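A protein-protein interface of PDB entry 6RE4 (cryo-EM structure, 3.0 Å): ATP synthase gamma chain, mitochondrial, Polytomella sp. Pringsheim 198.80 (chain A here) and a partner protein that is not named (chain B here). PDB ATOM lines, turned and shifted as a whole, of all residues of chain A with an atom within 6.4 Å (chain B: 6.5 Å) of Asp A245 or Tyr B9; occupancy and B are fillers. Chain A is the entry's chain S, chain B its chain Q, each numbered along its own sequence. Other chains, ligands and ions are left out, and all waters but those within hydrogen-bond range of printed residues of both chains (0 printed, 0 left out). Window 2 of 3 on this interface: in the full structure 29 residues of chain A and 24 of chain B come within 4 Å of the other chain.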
ATOM      1  N   PRO A 213     -30.051  28.768  23.332  1.00  0.00           N
ATOM      2  CA  PRO A 213     -28.594  28.914  23.503  1.00  0.00           C
ATOM      3  C   PRO A 213     -28.082  30.191  24.152  1.00  0.00           C
ATOM      4  O   PRO A 213     -27.705  30.153  25.323  1.00  0.00           O
ATOM      5  CB  PRO A 213     -28.077  28.820  22.063  1.00  0.00           C
ATOM      6  CG  PRO A 213     -29.241  29.114  21.206  1.00  0.00           C
ATOM      7  CD  PRO A 213     -30.393  28.538  21.919  1.00  0.00           C
ATOM      8  N   SER A 240     -22.341  31.560  19.423  1.00  0.00           N
ATOM      9  CA  SER A 240     -23.794  31.479  19.428  1.00  0.00           C
ATOM     10  C   SER A 240     -24.286  30.445  18.430  1.00  0.00           C
ATOM     11  O   SER A 240     -25.260  29.738  18.698  1.00  0.00           O
ATOM     12  CB  SER A 240     -24.390  32.849  19.132  1.00  0.00           C
ATOM     13  OG  SER A 240     -23.770  33.435  18.007  1.00  0.00           O
ATOM     14  N   ASP A 241     -23.598  30.302  17.299  1.00  0.00           N
ATOM     15  CA  ASP A 241     -24.028  29.321  16.310  1.00  0.00           C
ATOM     16  C   ASP A 241     -23.701  27.903  16.757  1.00  0.00           C
ATOM     17  O   ASP A 241     -24.511  26.983  16.565  1.00  0.00           O
ATOM     18  CB  ASP A 241     -23.404  29.638  14.956  1.00  0.00           C
ATOM     19  CG  ASP A 241     -23.730  31.048  14.478  1.00  0.00           C
ATOM     20  OD1 ASP A 241     -24.668  31.668  15.019  1.00  0.00           O
ATOM     21  OD2 ASP A 241     -23.064  31.537  13.547  1.00  0.00           O
ATOM     22  N   VAL A 242     -22.546  27.706  17.397  1.00  0.00           N
ATOM     23  CA  VAL A 242     -22.223  26.374  17.891  1.00  0.00           C
ATOM     24  C   VAL A 242     -23.086  26.029  19.097  1.00  0.00           C
ATOM     25  O   VAL A 242     -23.427  24.864  19.296  1.00  0.00           O
ATOM     26  CB  VAL A 242     -20.713  26.241  18.182  1.00  0.00           C
ATOM     27  CG1 VAL A 242     -20.313  26.905  19.458  1.00  0.00           C
ATOM     28  CG2 VAL A 242     -20.308  24.795  18.234  1.00  0.00           C
ATOM     29  N   LEU A 243     -23.540  27.023  19.864  1.00  0.00           N
ATOM     30  CA  LEU A 243     -24.439  26.728  20.970  1.00  0.00           C
ATOM     31  C   LEU A 243     -25.854  26.478  20.500  1.00  0.00           C
ATOM     32  O   LEU A 243     -26.566  25.690  21.120  1.00  0.00           O
ATOM     33  CB  LEU A 243     -24.442  27.856  21.989  1.00  0.00           C
ATOM     34  CG  LEU A 243     -23.721  27.572  23.296  1.00  0.00           C
ATOM     35  CD1 LEU A 243     -22.229  27.560  23.107  1.00  0.00           C
ATOM     36  CD2 LEU A 243     -24.131  28.612  24.287  1.00  0.00           C
ATOM     37  N   ARG A 244     -26.273  27.125  19.410  1.00  0.00           N
ATOM     38  CA  ARG A 244     -27.547  26.799  18.784  1.00  0.00           C
ATOM     39  C   ARG A 244     -27.553  25.364  18.283  1.00  0.00           C
ATOM     40  O   ARG A 244     -28.488  24.601  18.559  1.00  0.00           O
ATOM     41  CB  ARG A 244     -27.811  27.775  17.640  1.00  0.00           C
ATOM     42  CG  ARG A 244     -28.964  27.414  16.732  1.00  0.00           C
ATOM     43  CD  ARG A 244     -30.276  27.914  17.297  1.00  0.00           C
ATOM     44  NE  ARG A 244     -30.252  29.354  17.532  1.00  0.00           N
ATOM     45  CZ  ARG A 244     -31.215  30.022  18.155  1.00  0.00           C
ATOM     46  NH1 ARG A 244     -31.114  31.329  18.328  1.00  0.00           N
ATOM     47  NH2 ARG A 244     -32.278  29.378  18.608  1.00  0.00           N
ATOM     48  N   ASP A 245     -26.481  24.964  17.592  1.00  0.00           N
ATOM     49  CA  ASP A 245     -26.386  23.593  17.095  1.00  0.00           C
ATOM     50  C   ASP A 245     -26.265  22.591  18.238  1.00  0.00           C
ATOM     51  O   ASP A 245     -26.831  21.494  18.172  1.00  0.00           O
ATOM     52  CB  ASP A 245     -25.200  23.463  16.150  1.00  0.00           C
ATOM     53  CG  ASP A 245     -25.339  24.335  14.926  1.00  0.00           C
ATOM     54  OD1 ASP A 245     -26.485  24.643  14.544  1.00  0.00           O
ATOM     55  OD2 ASP A 245     -24.304  24.711  14.335  1.00  0.00           O
ATOM     56  N   LEU A 246     -25.578  22.972  19.313  1.00  0.00           N
ATOM     57  CA  LEU A 246     -25.433  22.089  20.461  1.00  0.00           C
ATOM     58  C   LEU A 246     -26.747  21.909  21.200  1.00  0.00           C
ATOM     59  O   LEU A 246     -27.043  20.813  21.670  1.00  0.00           O
ATOM     60  CB  LEU A 246     -24.380  22.635  21.412  1.00  0.00           C
ATOM     61  CG  LEU A 246     -22.970  22.103  21.236  1.00  0.00           C
ATOM     62  CD1 LEU A 246     -22.075  22.707  22.275  1.00  0.00           C
ATOM     63  CD2 LEU A 246     -23.009  20.633  21.397  1.00  0.00           C
ATOM     64  N   THR A 247     -27.546  22.966  21.320  1.00  0.00           N
ATOM     65  CA  THR A 247     -28.820  22.826  22.009  1.00  0.00           C
ATOM     66  C   THR A 247     -29.820  22.044  21.176  1.00  0.00           C
ATOM     67  O   THR A 247     -30.624  21.293  21.731  1.00  0.00           O
ATOM     68  CB  THR A 247     -29.381  24.186  22.384  1.00  0.00           C
ATOM     69  OG1 THR A 247     -29.278  25.073  21.270  1.00  0.00           O
ATOM     70  CG2 THR A 247     -28.594  24.736  23.536  1.00  0.00           C
ATOM     71  N   GLU A 248     -29.780  22.193  19.848  1.00  0.00           N
ATOM     72  CA  GLU A 248     -30.618  21.339  19.007  1.00  0.00           C
ATOM     73  C   GLU A 248     -30.212  19.876  19.126  1.00  0.00           C
ATOM     74  O   GLU A 248     -31.070  18.997  19.244  1.00  0.00           O
ATOM     75  CB  GLU A 248     -30.551  21.794  17.555  1.00  0.00           C
ATOM     76  CG  GLU A 248     -31.138  23.169  17.335  1.00  0.00           C
ATOM     77  CD  GLU A 248     -31.056  23.638  15.897  1.00  0.00           C
ATOM     78  OE1 GLU A 248     -30.477  22.914  15.065  1.00  0.00           O
ATOM     79  OE2 GLU A 248     -31.559  24.743  15.602  1.00  0.00           O
ATOM     80  N   PHE A 249     -28.909  19.603  19.173  1.00  0.00           N
ATOM     81  CA  PHE A 249     -28.441  18.228  19.294  1.00  0.00           C
ATOM     82  C   PHE A 249     -28.730  17.665  20.680  1.00  0.00           C
ATOM     83  O   PHE A 249     -29.056  16.482  20.821  1.00  0.00           O
ATOM     84  CB  PHE A 249     -26.958  18.195  18.944  1.00  0.00           C
ATOM     85  CG  PHE A 249     -26.362  16.835  18.883  1.00  0.00           C
ATOM     86  CD1 PHE A 249     -27.017  15.799  18.266  1.00  0.00           C
ATOM     87  CD2 PHE A 249     -25.073  16.630  19.321  1.00  0.00           C
ATOM     88  CE1 PHE A 249     -26.436  14.562  18.189  1.00  0.00           C
ATOM     89  CE2 PHE A 249     -24.492  15.398  19.245  1.00  0.00           C
ATOM     90  CZ  PHE A 249     -25.171  14.367  18.673  1.00  0.00           C
ATOM     91  N   HIS A 250     -28.696  18.517  21.702  1.00  0.00           N
ATOM     92  CA  HIS A 250     -29.000  18.080  23.059  1.00  0.00           C
ATOM     93  C   HIS A 250     -30.478  17.779  23.219  1.00  0.00           C
ATOM     94  O   HIS A 250     -30.850  16.790  23.855  1.00  0.00           O
ATOM     95  CB  HIS A 250     -28.548  19.148  24.051  1.00  0.00           C
ATOM     96  CG  HIS A 250     -29.019  18.927  25.452  1.00  0.00           C
ATOM     97  ND1 HIS A 250     -29.039  17.685  26.044  1.00  0.00           N
ATOM     98  CD2 HIS A 250     -29.400  19.803  26.409  1.00  0.00           C
ATOM     99  CE1 HIS A 250     -29.457  17.800  27.290  1.00  0.00           C
ATOM    100  NE2 HIS A 250     -29.682  19.075  27.536  1.00  0.00           N
ATOM    101  N   GLY B   6     -24.867  32.043   9.797  1.00  0.00           N
ATOM    102  CA  GLY B   6     -24.266  30.963  10.536  1.00  0.00           C
ATOM    103  C   GLY B   6     -23.509  30.046   9.606  1.00  0.00           C
ATOM    104  O   GLY B   6     -22.889  30.489   8.637  1.00  0.00           O
ATOM    105  N   PRO B   7     -23.540  28.751   9.872  1.00  0.00           N
ATOM    106  CA  PRO B   7     -22.910  27.800   8.954  1.00  0.00           C
ATOM    107  C   PRO B   7     -23.673  27.621   7.657  1.00  0.00           C
ATOM    108  O   PRO B   7     -24.709  28.256   7.451  1.00  0.00           O
ATOM    109  CB  PRO B   7     -22.883  26.509   9.770  1.00  0.00           C
ATOM    110  CG  PRO B   7     -22.958  26.951  11.169  1.00  0.00           C
ATOM    111  CD  PRO B   7     -23.845  28.131  11.164  1.00  0.00           C
ATOM    112  N   PHE B   8     -23.189  26.750   6.773  1.00  0.00           N
ATOM    113  CA  PHE B   8     -23.800  26.652   5.456  1.00  0.00           C
ATOM    114  C   PHE B   8     -25.132  25.921   5.475  1.00  0.00           C
ATOM    115  O   PHE B   8     -25.852  25.960   4.476  1.00  0.00           O
ATOM    116  CB  PHE B   8     -22.848  25.983   4.467  1.00  0.00           C
ATOM    117  CG  PHE B   8     -22.804  24.492   4.558  1.00  0.00           C
ATOM    118  CD1 PHE B   8     -23.418  23.711   3.600  1.00  0.00           C
ATOM    119  CD2 PHE B   8     -22.113  23.870   5.576  1.00  0.00           C
ATOM    120  CE1 PHE B   8     -23.366  22.345   3.674  1.00  0.00           C
ATOM    121  CE2 PHE B   8     -22.057  22.496   5.649  1.00  0.00           C
ATOM    122  CZ  PHE B   8     -22.685  21.735   4.696  1.00  0.00           C
ATOM    123  N   TYR B   9     -25.471  25.243   6.566  1.00  0.00           N
ATOM    124  CA  TYR B   9     -26.817  24.711   6.694  1.00  0.00           C
ATOM    125  C   TYR B   9     -27.754  25.741   7.304  1.00  0.00           C
ATOM    126  O   TYR B   9     -28.923  25.829   6.919  1.00  0.00           O
ATOM    127  CB  TYR B   9     -26.808  23.424   7.523  1.00  0.00           C
ATOM    128  CG  TYR B   9     -26.002  23.480   8.797  1.00  0.00           C
ATOM    129  CD1 TYR B   9     -24.695  23.035   8.830  1.00  0.00           C
ATOM    130  CD2 TYR B   9     -26.558  23.950   9.970  1.00  0.00           C
ATOM    131  CE1 TYR B   9     -23.965  23.081   9.985  1.00  0.00           C
ATOM    132  CE2 TYR B   9     -25.834  24.002  11.128  1.00  0.00           C
ATOM    133  CZ  TYR B   9     -24.541  23.565  11.128  1.00  0.00           C
ATOM    134  OH  TYR B   9     -23.817  23.613  12.287  1.00  0.00           O
ATOM    135  N   ARG B  10     -27.247  26.546   8.231  1.00  0.00           N
ATOM    136  CA  ARG B  10     -28.085  27.502   8.934  1.00  0.00           C
ATOM    137  C   ARG B  10     -28.479  28.660   8.036  1.00  0.00           C
ATOM    138  O   ARG B  10     -29.578  29.202   8.174  1.00  0.00           O
ATOM    139  CB  ARG B  10     -27.351  28.009  10.169  1.00  0.00           C
ATOM    140  CG  ARG B  10     -28.171  28.850  11.104  1.00  0.00           C
ATOM    141  CD  ARG B  10     -29.268  28.037  11.738  1.00  0.00           C
ATOM    142  NE  ARG B  10     -28.761  26.831  12.371  1.00  0.00           N
ATOM    143  CZ  ARG B  10     -29.439  26.140  13.274  1.00  0.00           C
ATOM    144  NH1 ARG B  10     -30.639  26.550  13.645  1.00  0.00           N
ATOM    145  NH2 ARG B  10     -28.921  25.047  13.811  1.00  0.00           N
ATOM    146  N   VAL B  11     -27.608  29.040   7.097  1.00  0.00           N
ATOM    147  CA  VAL B  11     -27.967  30.060   6.118  1.00  0.00           C
ATOM    148  C   VAL B  11     -28.809  29.505   4.987  1.00  0.00           C
ATOM    149  O   VAL B  11     -29.304  30.281   4.163  1.00  0.00           O
ATOM    150  CB  VAL B  11     -26.731  30.731   5.492  1.00  0.00           C
ATOM    151  CG1 VAL B  11     -25.817  31.279   6.570  1.00  0.00           C
ATOM    152  CG2 VAL B  11     -25.998  29.750   4.602  1.00  0.00           C
ATOM    153  N   ALA B  12     -28.983  28.187   4.915  1.00  0.00           N
ATOM    154  CA  ALA B  12     -29.848  27.561   3.930  1.00  0.00           C
ATOM    155  C   ALA B  12     -31.183  27.145   4.522  1.00  0.00           C
ATOM    156  O   ALA B  12     -31.890  26.333   3.920  1.00  0.00           O
ATOM    157  CB  ALA B  12     -29.156  26.353   3.307  1.00  0.00           C
ATOM    158  N   GLY B  13     -31.534  27.671   5.693  1.00  0.00           N
ATOM    159  CA  GLY B  13     -32.792  27.330   6.326  1.00  0.00           C
ATOM    160  C   GLY B  13     -32.865  25.932   6.890  1.00  0.00           C
ATOM    161  O   GLY B  13     -33.965  25.427   7.122  1.00  0.00           O
ATOM    162  N   MET B  14     -31.724  25.296   7.130  1.00  0.00           N
ATOM    163  CA  MET B  14     -31.652  23.919   7.595  1.00  0.00           C
ATOM    164  C   MET B  14     -31.049  23.890   8.989  1.00  0.00           C
ATOM    165  O   MET B  14     -29.962  24.426   9.208  1.00  0.00           O
ATOM    166  CB  MET B  14     -30.811  23.087   6.632  1.00  0.00           C
ATOM    167  CG  MET B  14     -30.493  21.704   7.089  1.00  0.00           C
ATOM    168  SD  MET B  14     -29.299  20.945   5.985  1.00  0.00           S
ATOM    169  CE  MET B  14     -30.102  21.161   4.417  1.00  0.00           C
ATOM    170  N   SER B  15     -31.748  23.266   9.932  1.00  0.00           N
ATOM    171  CA  SER B  15     -31.246  23.192  11.294  1.00  0.00           C
ATOM    172  C   SER B  15     -30.123  22.167  11.391  1.00  0.00           C
ATOM    173  O   SER B  15     -29.832  21.438  10.443  1.00  0.00           O
ATOM    174  CB  SER B  15     -32.370  22.848  12.265  1.00  0.00           C
ATOM    175  OG  SER B  15     -32.930  21.588  11.963  1.00  0.00           O
ATOM    176  N   TYR B  16     -29.485  22.118  12.562  1.00  0.00           N
ATOM    177  CA  TYR B  16     -28.331  21.245  12.726  1.00  0.00           C
ATOM    178  C   TYR B  16     -28.724  19.782  12.720  1.00  0.00           C
ATOM    179  O   TYR B  16     -27.986  18.948  12.184  1.00  0.00           O
ATOM    180  CB  TYR B  16     -27.599  21.548  14.027  1.00  0.00           C
ATOM    181  CG  TYR B  16     -26.442  20.608  14.240  1.00  0.00           C
ATOM    182  CD1 TYR B  16     -25.309  20.704  13.451  1.00  0.00           C
ATOM    183  CD2 TYR B  16     -26.493  19.603  15.196  1.00  0.00           C
ATOM    184  CE1 TYR B  16     -24.260  19.855  13.616  1.00  0.00           C
ATOM    185  CE2 TYR B  16     -25.444  18.740  15.358  1.00  0.00           C
ATOM    186  CZ  TYR B  16     -24.330  18.878  14.565  1.00  0.00           C
ATOM    187  OH  TYR B  16     -23.271  18.030  14.719  1.00  0.00           O
ATOM    188  N   LEU B  17     -29.867  19.461  13.328  1.00  0.00           N
ATOM    189  CA  LEU B  17     -30.307  18.079  13.420  1.00  0.00           C
ATOM    190  C   LEU B  17     -30.609  17.505  12.053  1.00  0.00           C
ATOM    191  O   LEU B  17     -30.229  16.369  11.762  1.00  0.00           O
ATOM    192  CB  LEU B  17     -31.531  17.983  14.311  1.00  0.00           C
ATOM    193  CG  LEU B  17     -31.199  17.843  15.781  1.00  0.00           C
ATOM    194  CD1 LEU B  17     -32.479  17.895  16.520  1.00  0.00           C
ATOM    195  CD2 LEU B  17     -30.489  16.534  16.032  1.00  0.00           C
ATOM    196  N   TYR B  19     -29.245  18.557   9.212  1.00  0.00           N
ATOM    197  CA  TYR B  19     -27.994  18.466   8.470  1.00  0.00           C
ATOM    198  C   TYR B  19     -27.195  17.242   8.888  1.00  0.00           C
ATOM    199  O   TYR B  19     -26.707  16.481   8.044  1.00  0.00           O
ATOM    200  CB  TYR B  19     -27.181  19.740   8.676  1.00  0.00           C
ATOM    201  CG  TYR B  19     -25.686  19.574   8.581  1.00  0.00           C
ATOM    202  CD1 TYR B  19     -24.898  19.591   9.725  1.00  0.00           C
ATOM    203  CD2 TYR B  19     -25.059  19.434   7.353  1.00  0.00           C
ATOM    204  CE1 TYR B  19     -23.539  19.447   9.650  1.00  0.00           C
ATOM    205  CE2 TYR B  19     -23.694  19.292   7.273  1.00  0.00           C
ATOM    206  CZ  TYR B  19     -22.941  19.302   8.427  1.00  0.00           C
ATOM    207  OH  TYR B  19     -21.577  19.164   8.362  1.00  0.00           O
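The side-chain hydroxyl of Tyr B9 sits close to the side-chain carboxylate of Asp A245.
The guanidinium group (NH2) of Arg B10 is in salt-bridge range of the side-chain carboxylate (OD1) of Asp A245.
The side-chain carboxylate (OE1) of Glu A248 lies within hydrogen-bond range of the backbone NH (N) of Tyr B16.
NH1 of Arg B10 lies within salt-bridge range of OE2 of Glu A248 (2.8 Å).
O of Tyr B9 lies within hydrogen-bond range of N of Met B14 (2.9 Å).
The backbone carbonyl oxygen (O) of Arg A244 is in hydrogen-bond range of the side-chain hydroxyl (OG1) of Thr A247, at 2.9 Å.
Among the printed residues, merely in contact across the chains: Glu A248 with Leu B17 (3.3 Å), Asp A241 with Gly B6 (3.3 Å), Asp A245 with Tyr B16 (3.3 Å), Glu A248 with Ser B15 (3.4 Å), Arg A244 with Arg B10 (3.6 Å) and Phe A249 with Tyr B16 (3.9 Å).
Of the printed residues of chain B, Asp A241 touches Gly B6 (3.3 Å).
Leu A243 touches none of the printed residues of chain B.
Asp A245 touches just these residues of chain B: Tyr B9, Arg B10 and Tyr B16.
Of the printed residues of chain B, Glu A248 touches Arg B10 (2.8 Å), Ser B15 (3.4 Å), Tyr B16 (2.8 Å) and Leu B17 (3.3 Å).
Printed residues of chain A within 4 Å of Gly B6: Asp A241 (3.3 Å).
Tyr B9 touches one residue of chain A.
Val B11 touches none of the printed residues of chain A.
Of the printed residues of chain A, Ser B15 touches Glu A248.
Of the printed residues of chain A, Leu B17 touches Glu A248 (3.3 Å).
The nearest residue of chain A that does not touch Tyr B9 is Asp A241 (5.5 Å).
The nearest printed residue of chain B that does not touch Phe A249 is Leu B17 (4.2 Å).
Of the 13 printed residues of chain B, 6 touch a printed residue of chain A.
Printed residues of chain B that touch a printed residue of chain A: Gly B6, Tyr B9, Arg B10, Ser B15, Tyr B16 and Leu B17.
Printed residues of chain A that touch a printed residue of chain B: Asp A241, Arg A244, Asp A245, Glu A248 and Phe A249.
Along chain A the printed residues that touch a printed residue of chain B span positions 241 to 249.
Among the printed residues, 10 pairs touch across the chains.
Among the printed residues, Asp or Glu carboxylates within 4 Å of a Lys or Arg side-chain nitrogen of the other chain: Asp A245 with Arg B10 (2.6 Å) and Glu A248 with Arg B10 (2.8 Å).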
